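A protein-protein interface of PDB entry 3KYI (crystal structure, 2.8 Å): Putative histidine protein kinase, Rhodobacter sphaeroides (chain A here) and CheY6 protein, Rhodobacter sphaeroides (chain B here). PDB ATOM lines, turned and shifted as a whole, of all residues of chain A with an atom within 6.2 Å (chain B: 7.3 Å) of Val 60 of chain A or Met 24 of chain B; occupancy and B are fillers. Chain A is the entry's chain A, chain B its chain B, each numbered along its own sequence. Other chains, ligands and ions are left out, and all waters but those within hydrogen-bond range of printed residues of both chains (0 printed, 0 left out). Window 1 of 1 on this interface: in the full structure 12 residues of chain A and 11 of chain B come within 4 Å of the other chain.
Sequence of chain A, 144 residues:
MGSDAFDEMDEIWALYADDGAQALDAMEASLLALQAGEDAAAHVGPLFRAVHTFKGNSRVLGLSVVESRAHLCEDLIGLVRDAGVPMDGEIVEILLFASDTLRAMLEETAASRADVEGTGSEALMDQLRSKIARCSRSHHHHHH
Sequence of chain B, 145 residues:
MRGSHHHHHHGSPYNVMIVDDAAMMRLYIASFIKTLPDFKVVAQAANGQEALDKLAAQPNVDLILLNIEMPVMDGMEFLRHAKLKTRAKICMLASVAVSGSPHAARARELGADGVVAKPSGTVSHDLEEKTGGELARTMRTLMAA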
ATOM      1  N   GLU A  11      29.557  -1.627  23.303  1.00  0.00           N
ATOM      2  CA  GLU A  11      28.949  -2.606  24.211  1.00  0.00           C
ATOM      3  C   GLU A  11      27.486  -2.886  23.851  1.00  0.00           C
ATOM      4  O   GLU A  11      27.029  -4.017  24.022  1.00  0.00           O
ATOM      5  CB  GLU A  11      29.069  -2.152  25.675  1.00  0.00           C
ATOM      6  CG  GLU A  11      29.025  -3.303  26.671  1.00  0.00           C
ATOM      7  CD  GLU A  11      28.851  -2.926  28.131  1.00  0.00           C
ATOM      8  OE1 GLU A  11      29.636  -2.089  28.635  1.00  0.00           O
ATOM      9  OE2 GLU A  11      27.958  -3.509  28.787  1.00  0.00           O
ATOM     10  N   ILE A  12      26.759  -1.856  23.363  1.00  0.00           N
ATOM     11  CA  ILE A  12      25.350  -1.946  22.962  1.00  0.00           C
ATOM     12  C   ILE A  12      25.141  -2.934  21.795  1.00  0.00           C
ATOM     13  O   ILE A  12      24.220  -3.751  21.843  1.00  0.00           O
ATOM     14  CB  ILE A  12      24.725  -0.526  22.761  1.00  0.00           C
ATOM     15  CG1 ILE A  12      23.398  -0.371  23.516  1.00  0.00           C
ATOM     16  CG2 ILE A  12      24.612  -0.080  21.292  1.00  0.00           C
ATOM     17  CD1 ILE A  12      23.234   0.986  24.184  1.00  0.00           C
ATOM     18  N   TRP A  13      26.040  -2.889  20.788  1.00  0.00           N
ATOM     19  CA  TRP A  13      26.020  -3.766  19.617  1.00  0.00           C
ATOM     20  C   TRP A  13      26.465  -5.178  19.974  1.00  0.00           C
ATOM     21  O   TRP A  13      25.962  -6.140  19.388  1.00  0.00           O
ATOM     22  CB  TRP A  13      26.876  -3.185  18.485  1.00  0.00           C
ATOM     23  CG  TRP A  13      26.159  -2.116  17.719  1.00  0.00           C
ATOM     24  CD1 TRP A  13      26.275  -0.768  17.888  1.00  0.00           C
ATOM     25  CD2 TRP A  13      25.144  -2.312  16.727  1.00  0.00           C
ATOM     26  NE1 TRP A  13      25.422  -0.109  17.034  1.00  0.00           N
ATOM     27  CE2 TRP A  13      24.715  -1.034  16.310  1.00  0.00           C
ATOM     28  CE3 TRP A  13      24.562  -3.448  16.140  1.00  0.00           C
ATOM     29  CZ2 TRP A  13      23.734  -0.858  15.324  1.00  0.00           C
ATOM     30  CZ3 TRP A  13      23.586  -3.274  15.171  1.00  0.00           C
ATOM     31  CH2 TRP A  13      23.185  -1.993  14.769  1.00  0.00           C
ATOM     32  N   LEU A  15      25.952  -6.523  22.931  1.00  0.00           N
ATOM     33  CA  LEU A  15      24.798  -7.017  23.677  1.00  0.00           C
ATOM     34  C   LEU A  15      23.685  -7.423  22.719  1.00  0.00           C
ATOM     35  O   LEU A  15      22.986  -8.395  22.988  1.00  0.00           O
ATOM     36  CB  LEU A  15      24.305  -5.945  24.660  1.00  0.00           C
ATOM     37  CG  LEU A  15      24.571  -6.184  26.151  1.00  0.00           C
ATOM     38  CD1 LEU A  15      26.064  -6.260  26.460  1.00  0.00           C
ATOM     39  CD2 LEU A  15      23.957  -5.081  26.983  1.00  0.00           C
ATOM     40  N   TYR A  16      23.542  -6.695  21.590  1.00  0.00           N
ATOM     41  CA  TYR A  16      22.557  -6.973  20.540  1.00  0.00           C
ATOM     42  C   TYR A  16      22.867  -8.318  19.870  1.00  0.00           C
ATOM     43  O   TYR A  16      21.948  -9.088  19.588  1.00  0.00           O
ATOM     44  CB  TYR A  16      22.520  -5.812  19.519  1.00  0.00           C
ATOM     45  CG  TYR A  16      21.806  -6.127  18.220  1.00  0.00           C
ATOM     46  CD1 TYR A  16      20.416  -6.157  18.155  1.00  0.00           C
ATOM     47  CD2 TYR A  16      22.520  -6.363  17.049  1.00  0.00           C
ATOM     48  CE1 TYR A  16      19.753  -6.452  16.962  1.00  0.00           C
ATOM     49  CE2 TYR A  16      21.870  -6.654  15.850  1.00  0.00           C
ATOM     50  CZ  TYR A  16      20.486  -6.706  15.813  1.00  0.00           C
ATOM     51  OH  TYR A  16      19.843  -6.984  14.630  1.00  0.00           O
ATOM     52  N   ALA A  17      24.165  -8.598  19.644  1.00  0.00           N
ATOM     53  CA  ALA A  17      24.657  -9.839  19.052  1.00  0.00           C
ATOM     54  C   ALA A  17      24.463 -11.003  20.023  1.00  0.00           C
ATOM     55  O   ALA A  17      24.116 -12.102  19.592  1.00  0.00           O
ATOM     56  CB  ALA A  17      26.128  -9.698  18.691  1.00  0.00           C
ATOM     57  N   ASP A  19      22.201 -11.084  22.970  1.00  0.00           N
ATOM     58  CA  ASP A  19      20.764 -11.250  23.208  1.00  0.00           C
ATOM     59  C   ASP A  19      20.042 -11.790  21.974  1.00  0.00           C
ATOM     60  O   ASP A  19      19.149 -12.626  22.113  1.00  0.00           O
ATOM     61  CB  ASP A  19      20.115  -9.939  23.684  1.00  0.00           C
ATOM     62  CG  ASP A  19      20.552  -9.463  25.057  1.00  0.00           C
ATOM     63  OD1 ASP A  19      21.050  -8.321  25.157  1.00  0.00           O
ATOM     64  OD2 ASP A  19      20.341 -10.209  26.042  1.00  0.00           O
ATOM     65  N   LYS A  55      12.699  -8.539  18.198  1.00  0.00           N
ATOM     66  CA  LYS A  55      12.025  -7.402  17.565  1.00  0.00           C
ATOM     67  C   LYS A  55      12.260  -6.119  18.374  1.00  0.00           C
ATOM     68  O   LYS A  55      12.450  -5.058  17.784  1.00  0.00           O
ATOM     69  CB  LYS A  55      10.515  -7.675  17.413  1.00  0.00           C
ATOM     70  CG  LYS A  55       9.768  -6.663  16.535  1.00  0.00           C
ATOM     71  CD  LYS A  55       8.254  -6.710  16.724  1.00  0.00           C
ATOM     72  CE  LYS A  55       7.774  -5.903  17.910  1.00  0.00           C
ATOM     73  NZ  LYS A  55       6.322  -6.096  18.156  1.00  0.00           N
ATOM     74  N   GLY A  56      12.254  -6.244  19.703  1.00  0.00           N
ATOM     75  CA  GLY A  56      12.464  -5.144  20.640  1.00  0.00           C
ATOM     76  C   GLY A  56      13.842  -4.515  20.570  1.00  0.00           C
ATOM     77  O   GLY A  56      13.958  -3.284  20.613  1.00  0.00           O
ATOM     78  N   ASN A  57      14.896  -5.358  20.470  1.00  0.00           N
ATOM     79  CA  ASN A  57      16.299  -4.934  20.378  1.00  0.00           C
ATOM     80  C   ASN A  57      16.572  -4.227  19.051  1.00  0.00           C
ATOM     81  O   ASN A  57      17.265  -3.208  19.032  1.00  0.00           O
ATOM     82  CB  ASN A  57      17.245  -6.132  20.544  1.00  0.00           C
ATOM     83  CG  ASN A  57      17.398  -6.670  21.953  1.00  0.00           C
ATOM     84  OD1 ASN A  57      16.991  -6.063  22.955  1.00  0.00           O
ATOM     85  ND2 ASN A  57      18.029  -7.825  22.059  1.00  0.00           N
ATOM     86  N   SER A  58      16.016  -4.765  17.947  1.00  0.00           N
ATOM     87  CA  SER A  58      16.153  -4.212  16.600  1.00  0.00           C
ATOM     88  C   SER A  58      15.461  -2.854  16.477  1.00  0.00           C
ATOM     89  O   SER A  58      15.993  -1.964  15.818  1.00  0.00           O
ATOM     90  CB  SER A  58      15.612  -5.186  15.559  1.00  0.00           C
ATOM     91  OG  SER A  58      14.239  -5.465  15.778  1.00  0.00           O
ATOM     92  N   ARG A  59      14.294  -2.700  17.135  1.00  0.00           N
ATOM     93  CA  ARG A  59      13.502  -1.467  17.171  1.00  0.00           C
ATOM     94  C   ARG A  59      14.287  -0.354  17.878  1.00  0.00           C
ATOM     95  O   ARG A  59      14.202   0.805  17.471  1.00  0.00           O
ATOM     96  CB  ARG A  59      12.165  -1.719  17.896  1.00  0.00           C
ATOM     97  CG  ARG A  59      11.121  -0.618  17.710  1.00  0.00           C
ATOM     98  CD  ARG A  59      10.027  -0.680  18.764  1.00  0.00           C
ATOM     99  NE  ARG A  59       9.042  -1.729  18.487  1.00  0.00           N
ATOM    100  CZ  ARG A  59       7.729  -1.528  18.403  1.00  0.00           C
ATOM    101  NH1 ARG A  59       7.222  -0.313  18.583  1.00  0.00           N
ATOM    102  NH2 ARG A  59       6.912  -2.540  18.145  1.00  0.00           N
ATOM    103  N   VAL A  60      15.059  -0.721  18.919  1.00  0.00           N
ATOM    104  CA  VAL A  60      15.886   0.179  19.726  1.00  0.00           C
ATOM    105  C   VAL A  60      17.033   0.798  18.915  1.00  0.00           C
ATOM    106  O   VAL A  60      17.225   2.015  18.968  1.00  0.00           O
ATOM    107  CB  VAL A  60      16.341  -0.527  21.033  1.00  0.00           C
ATOM    108  CG1 VAL A  60      17.625   0.064  21.601  1.00  0.00           C
ATOM    109  CG2 VAL A  60      15.232  -0.495  22.072  1.00  0.00           C
ATOM    110  N   LEU A  61      17.762  -0.028  18.145  1.00  0.00           N
ATOM    111  CA  LEU A  61      18.877   0.435  17.314  1.00  0.00           C
ATOM    112  C   LEU A  61      18.427   1.015  15.956  1.00  0.00           C
ATOM    113  O   LEU A  61      19.267   1.454  15.159  1.00  0.00           O
ATOM    114  CB  LEU A  61      19.919  -0.683  17.125  1.00  0.00           C
ATOM    115  CG  LEU A  61      20.672  -1.162  18.367  1.00  0.00           C
ATOM    116  CD1 LEU A  61      21.413  -2.441  18.078  1.00  0.00           C
ATOM    117  CD2 LEU A  61      21.642  -0.106  18.884  1.00  0.00           C
ATOM    118  N   GLY A  62      17.114   1.030  15.726  1.00  0.00           N
ATOM    119  CA  GLY A  62      16.495   1.547  14.511  1.00  0.00           C
ATOM    120  C   GLY A  62      16.702   0.668  13.297  1.00  0.00           C
ATOM    121  O   GLY A  62      16.807   1.176  12.178  1.00  0.00           O
ATOM    122  N   LEU A  63      16.758  -0.659  13.509  1.00  0.00           N
ATOM    123  CA  LEU A  63      16.952  -1.655  12.449  1.00  0.00           C
ATOM    124  C   LEU A  63      15.583  -2.048  11.877  1.00  0.00           C
ATOM    125  O   LEU A  63      15.095  -3.159  12.100  1.00  0.00           O
ATOM    126  CB  LEU A  63      17.738  -2.884  12.982  1.00  0.00           C
ATOM    127  CG  LEU A  63      19.107  -2.603  13.601  1.00  0.00           C
ATOM    128  CD1 LEU A  63      19.375  -3.520  14.757  1.00  0.00           C
ATOM    129  CD2 LEU A  63      20.216  -2.709  12.581  1.00  0.00           C
ATOM    130  N   ASP B  20      13.986  -4.941  33.110  1.00  0.00           N
ATOM    131  CA  ASP B  20      13.723  -5.533  31.790  1.00  0.00           C
ATOM    132  C   ASP B  20      14.536  -6.819  31.630  1.00  0.00           C
ATOM    133  O   ASP B  20      15.694  -6.865  32.053  1.00  0.00           O
ATOM    134  CB  ASP B  20      14.058  -4.547  30.652  1.00  0.00           C
ATOM    135  CG  ASP B  20      13.592  -5.010  29.283  1.00  0.00           C
ATOM    136  OD1 ASP B  20      14.377  -5.686  28.587  1.00  0.00           O
ATOM    137  OD2 ASP B  20      12.441  -4.705  28.915  1.00  0.00           O
ATOM    138  N   ASP B  21      13.935  -7.851  31.007  1.00  0.00           N
ATOM    139  CA  ASP B  21      14.580  -9.152  30.790  1.00  0.00           C
ATOM    140  C   ASP B  21      15.726  -9.147  29.769  1.00  0.00           C
ATOM    141  O   ASP B  21      16.618  -9.996  29.857  1.00  0.00           O
ATOM    142  CB  ASP B  21      13.552 -10.271  30.511  1.00  0.00           C
ATOM    143  CG  ASP B  21      12.458  -9.944  29.508  1.00  0.00           C
ATOM    144  OD1 ASP B  21      12.591  -8.929  28.786  1.00  0.00           O
ATOM    145  OD2 ASP B  21      11.471 -10.706  29.439  1.00  0.00           O
ATOM    146  N   ALA B  22      15.718  -8.186  28.827  1.00  0.00           N
ATOM    147  CA  ALA B  22      16.766  -8.053  27.813  1.00  0.00           C
ATOM    148  C   ALA B  22      17.820  -7.032  28.254  1.00  0.00           C
ATOM    149  O   ALA B  22      17.493  -5.867  28.508  1.00  0.00           O
ATOM    150  CB  ALA B  22      16.163  -7.662  26.469  1.00  0.00           C
ATOM    151  N   ALA B  23      19.084  -7.495  28.370  1.00  0.00           N
ATOM    152  CA  ALA B  23      20.253  -6.712  28.790  1.00  0.00           C
ATOM    153  C   ALA B  23      20.485  -5.482  27.915  1.00  0.00           C
ATOM    154  O   ALA B  23      20.868  -4.426  28.426  1.00  0.00           O
ATOM    155  CB  ALA B  23      21.496  -7.591  28.793  1.00  0.00           C
ATOM    156  N   MET B  24      20.247  -5.631  26.597  1.00  0.00           N
ATOM    157  CA  MET B  24      20.388  -4.600  25.576  1.00  0.00           C
ATOM    158  C   MET B  24      19.514  -3.376  25.880  1.00  0.00           C
ATOM    159  O   MET B  24      20.002  -2.245  25.812  1.00  0.00           O
ATOM    160  CB  MET B  24      20.042  -5.186  24.201  1.00  0.00           C
ATOM    161  CG  MET B  24      21.042  -4.835  23.134  1.00  0.00           C
ATOM    162  SD  MET B  24      20.949  -3.122  22.579  1.00  0.00           S
ATOM    163  CE  MET B  24      19.597  -3.229  21.448  1.00  0.00           C
ATOM    164  N   MET B  25      18.237  -3.616  26.246  1.00  0.00           N
ATOM    165  CA  MET B  25      17.257  -2.589  26.602  1.00  0.00           C
ATOM    166  C   MET B  25      17.699  -1.832  27.862  1.00  0.00           C
ATOM    167  O   MET B  25      17.632  -0.602  27.886  1.00  0.00           O
ATOM    168  CB  MET B  25      15.869  -3.229  26.806  1.00  0.00           C
ATOM    169  CG  MET B  25      14.750  -2.226  27.076  1.00  0.00           C
ATOM    170  SD  MET B  25      14.310  -1.200  25.650  1.00  0.00           S
ATOM    171  CE  MET B  25      13.485  -2.434  24.620  1.00  0.00           C
ATOM    172  N   ARG B  26      18.163  -2.571  28.894  1.00  0.00           N
ATOM    173  CA  ARG B  26      18.642  -2.016  30.161  1.00  0.00           C
ATOM    174  C   ARG B  26      19.813  -1.067  29.934  1.00  0.00           C
ATOM    175  O   ARG B  26      19.843   0.009  30.530  1.00  0.00           O
ATOM    176  CB  ARG B  26      19.057  -3.128  31.133  1.00  0.00           C
ATOM    177  CG  ARG B  26      17.901  -3.943  31.707  1.00  0.00           C
ATOM    178  CD  ARG B  26      18.289  -4.671  32.986  1.00  0.00           C
ATOM    179  NE  ARG B  26      19.508  -5.475  32.850  1.00  0.00           N
ATOM    180  CZ  ARG B  26      19.544  -6.725  32.395  1.00  0.00           C
ATOM    181  NH1 ARG B  26      18.428  -7.334  32.014  1.00  0.00           N
ATOM    182  NH2 ARG B  26      20.699  -7.370  32.307  1.00  0.00           N
ATOM    183  N   LEU B  27      20.758  -1.459  29.047  1.00  0.00           N
ATOM    184  CA  LEU B  27      21.941  -0.674  28.701  1.00  0.00           C
ATOM    185  C   LEU B  27      21.588   0.584  27.917  1.00  0.00           C
ATOM    186  O   LEU B  27      22.197   1.624  28.158  1.00  0.00           O
ATOM    187  CB  LEU B  27      22.959  -1.524  27.930  1.00  0.00           C
ATOM    188  CG  LEU B  27      24.409  -1.045  28.003  1.00  0.00           C
ATOM    189  CD1 LEU B  27      25.125  -1.633  29.210  1.00  0.00           C
ATOM    190  CD2 LEU B  27      25.159  -1.406  26.747  1.00  0.00           C
ATOM    191  N   TYR B  28      20.605   0.497  26.992  1.00  0.00           N
ATOM    192  CA  TYR B  28      20.156   1.637  26.189  1.00  0.00           C
ATOM    193  C   TYR B  28      19.556   2.734  27.070  1.00  0.00           C
ATOM    194  O   TYR B  28      19.869   3.911  26.872  1.00  0.00           O
ATOM    195  CB  TYR B  28      19.180   1.198  25.084  1.00  0.00           C
ATOM    196  CG  TYR B  28      18.914   2.269  24.045  1.00  0.00           C
ATOM    197  CD1 TYR B  28      19.846   2.548  23.048  1.00  0.00           C
ATOM    198  CD2 TYR B  28      17.718   2.980  24.036  1.00  0.00           C
ATOM    199  CE1 TYR B  28      19.602   3.522  22.082  1.00  0.00           C
ATOM    200  CE2 TYR B  28      17.463   3.958  23.076  1.00  0.00           C
ATOM    201  CZ  TYR B  28      18.409   4.228  22.101  1.00  0.00           C
ATOM    202  OH  TYR B  28      18.165   5.197  21.156  1.00  0.00           O
ATOM    203  N   ILE B  29      18.736   2.334  28.065  1.00  0.00           N
ATOM    204  CA  ILE B  29      18.111   3.228  29.048  1.00  0.00           C
ATOM    205  C   ILE B  29      19.217   3.823  29.938  1.00  0.00           C
ATOM    206  O   ILE B  29      19.265   5.041  30.102  1.00  0.00           O
ATOM    207  CB  ILE B  29      16.987   2.497  29.852  1.00  0.00           C
ATOM    208  CG1 ILE B  29      15.819   2.087  28.921  1.00  0.00           C
ATOM    209  CG2 ILE B  29      16.473   3.354  31.028  1.00  0.00           C
ATOM    210  CD1 ILE B  29      15.016   0.871  29.375  1.00  0.00           C
ATOM    211  N   ALA B  30      20.142   2.965  30.442  1.00  0.00           N
ATOM    212  CA  ALA B  30      21.289   3.348  31.277  1.00  0.00           C
ATOM    213  C   ALA B  30      22.196   4.361  30.573  1.00  0.00           C
ATOM    214  O   ALA B  30      22.740   5.244  31.237  1.00  0.00           O
ATOM    215  CB  ALA B  30      22.092   2.117  31.670  1.00  0.00           C
ATOM    216  N   SER B  31      22.345   4.233  29.234  1.00  0.00           N
ATOM    217  CA  SER B  31      23.134   5.132  28.388  1.00  0.00           C
ATOM    218  C   SER B  31      22.452   6.498  28.285  1.00  0.00           C
ATOM    219  O   SER B  31      23.135   7.523  28.261  1.00  0.00           O
ATOM    220  CB  SER B  31      23.307   4.540  26.992  1.00  0.00           C
ATOM    221  OG  SER B  31      23.967   3.286  27.036  1.00  0.00           O
ATOM    222  N   SER B  95       6.861  -1.571  24.139  1.00  0.00           N
ATOM    223  CA  SER B  95       7.504  -1.495  22.822  1.00  0.00           C
ATOM    224  C   SER B  95       6.587  -0.901  21.749  1.00  0.00           C
ATOM    225  O   SER B  95       5.479  -1.388  21.530  1.00  0.00           O
ATOM    226  CB  SER B  95       8.015  -2.865  22.390  1.00  0.00           C
ATOM    227  OG  SER B  95       8.824  -3.475  23.383  1.00  0.00           O
ATOM    228  N   LYS B 118       8.826   2.531  24.855  1.00  0.00           N
ATOM    229  CA  LYS B 118      10.258   2.217  24.823  1.00  0.00           C
ATOM    230  C   LYS B 118      10.980   3.016  23.717  1.00  0.00           C
ATOM    231  O   LYS B 118      10.439   3.128  22.614  1.00  0.00           O
ATOM    232  CB  LYS B 118      10.492   0.708  24.687  1.00  0.00           C
ATOM    233  CG  LYS B 118      10.342  -0.035  26.007  1.00  0.00           C
ATOM    234  CD  LYS B 118      10.140  -1.521  25.797  1.00  0.00           C
ATOM    235  CE  LYS B 118      10.488  -2.323  27.025  1.00  0.00           C
ATOM    236  NZ  LYS B 118      10.708  -3.757  26.700  1.00  0.00           N
ATOM    237  N   PRO B 119      12.156   3.629  24.008  1.00  0.00           N
ATOM    238  CA  PRO B 119      12.830   4.458  22.987  1.00  0.00           C
ATOM    239  C   PRO B 119      13.335   3.724  21.748  1.00  0.00           C
ATOM    240  O   PRO B 119      13.580   2.517  21.790  1.00  0.00           O
ATOM    241  CB  PRO B 119      13.977   5.112  23.761  1.00  0.00           C
ATOM    242  CG  PRO B 119      14.243   4.192  24.890  1.00  0.00           C
ATOM    243  CD  PRO B 119      12.907   3.633  25.280  1.00  0.00           C
ATOM    244  N   SER B 120      13.483   4.472  20.642  1.00  0.00           N
ATOM    245  CA  SER B 120      13.966   3.971  19.357  1.00  0.00           C
ATOM    246  C   SER B 120      14.968   4.958  18.761  1.00  0.00           C
ATOM    247  O   SER B 120      14.675   6.152  18.663  1.00  0.00           O
ATOM    248  CB  SER B 120      12.800   3.742  18.399  1.00  0.00           C
ATOM    249  OG  SER B 120      12.057   4.930  18.181  1.00  0.00           O
ATOM    250  N   GLY B 121      16.142   4.450  18.393  1.00  0.00           N
ATOM    251  CA  GLY B 121      17.223   5.242  17.816  1.00  0.00           C
ATOM    252  C   GLY B 121      17.008   5.566  16.353  1.00  0.00           C
ATOM    253  O   GLY B 121      17.330   4.758  15.480  1.00  0.00           O
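OD1 of Asp 19 of chain A lies within hydrogen-bond range of N of Met 24 of chain B, 3.2 Å away. O of Val 60 of chain A is in hydrogen-bond range of N of Gly 121 of chain B (2.7 Å). SD of Met 24 of chain B sits close to O of Ile 12 of chain A (3.4 Å).
OD1 of Asp 20 of chain B is in hydrogen-bond range of N of Ala 22 of chain B (2.8 Å). OG of Ser 31 of chain B is in hydrogen-bond range of O of Leu 27 of chain B (2.7 Å).
Among the printed residues, merely in contact across the chains: Glu 11 of chain A with Leu 27 of chain B (3.4 Å), Ile 12 of chain A with Leu 27 of chain B (3.8 Å), Ile 12 of chain A with Tyr 28 of chain B (3.7 Å), Ile 12 of chain A with Ser 31 of chain B (3.7 Å), Leu 15 of chain A with Ala 23 of chain B (3.5 Å), Leu 15 of chain A with Met 24 of chain B (3.7 Å), Leu 15 of chain A with Leu 27 of chain B (3.8 Å), Tyr 16 of chain A with Met 24 of chain B (3.5 Å), Asp 19 of chain A with Ala 23 of chain B (3.7 Å), Asn 57 of chain A with Ala 22 of chain B (3.9 Å), Asn 57 of chain A with Met 24 of chain B (3.4 Å), Arg 59 of chain A with Ser 95 of chain B (3.3 Å), Arg 59 of chain A with Ser 120 of chain B (3.4 Å), Val 60 of chain A with Met 24 of chain B (3.8 Å), Val 60 of chain A with Met 25 of chain B (3.6 Å), Val 60 of chain A with Tyr 28 of chain B (3.5 Å), Val 60 of chain A with Pro 119 of chain B (3.4 Å), Val 60 of chain A with Ser 120 of chain B (3.7 Å), Leu 61 of chain A with Met 24 of chain B (3.9 Å), Leu 61 of chain A with Gly 121 of chain B (3.8 Å) and Gly 62 of chain A with Gly 121 of chain B (3.5 Å).
Printed residues of chain B within 4 Å of Asp 19 of chain A: Ala 23 (3.7 Å) and Met 24 (3.2 Å). Val 60 of chain A touches just these residues of chain B: Met 24 (3.8 Å), Met 25 (3.6 Å), Tyr 28 (3.5 Å), Pro 119 (3.4 Å), Ser 120 (3.7 Å) and Gly 121 (2.7 Å). Of the printed residues of chain B, Leu 61 of chain A touches Met 24 and Gly 121. Asp 20 of chain B touches none of the printed residues of chain A. Of the printed residues of chain A, Met 24 of chain B touches Ile 12, Leu 15, Tyr 16, Asp 19, Asn 57, Val 60 and Leu 61. Of the printed residues of chain A, Leu 27 of chain B touches Glu 11, Ile 12 and Leu 15. Ile 29 of chain B touches none of the printed residues of chain A. The nearest residue of chain A that does not touch Met 24 of chain B is Ser 58 of chain A (5.2 Å). The nearest printed residue of chain A that does not touch Ser 95 of chain B is Gly 56 of chain A (4.9 Å).
Of the 17 printed residues of chain B, 11 touch a printed residue of chain A. Printed residues of chain B that touch a printed residue of chain A: Ala 22, Ala 23, Met 24, Met 25, Leu 27, Tyr 28, Ser 31, Ser 95, Pro 119, Ser 120 and Gly 121. Of the 16 printed residues of chain A, 10 touch a printed residue of chain B. Hydrophobic or aromatic side chains of chain A within 4 Å of the printed part of chain B: Ile 12, Leu 15, Val 60 and Leu 61. Among the printed residues, no Asp or Glu carboxylate lies within 4 Å of a Lys or Arg side-chain nitrogen of the other chain.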
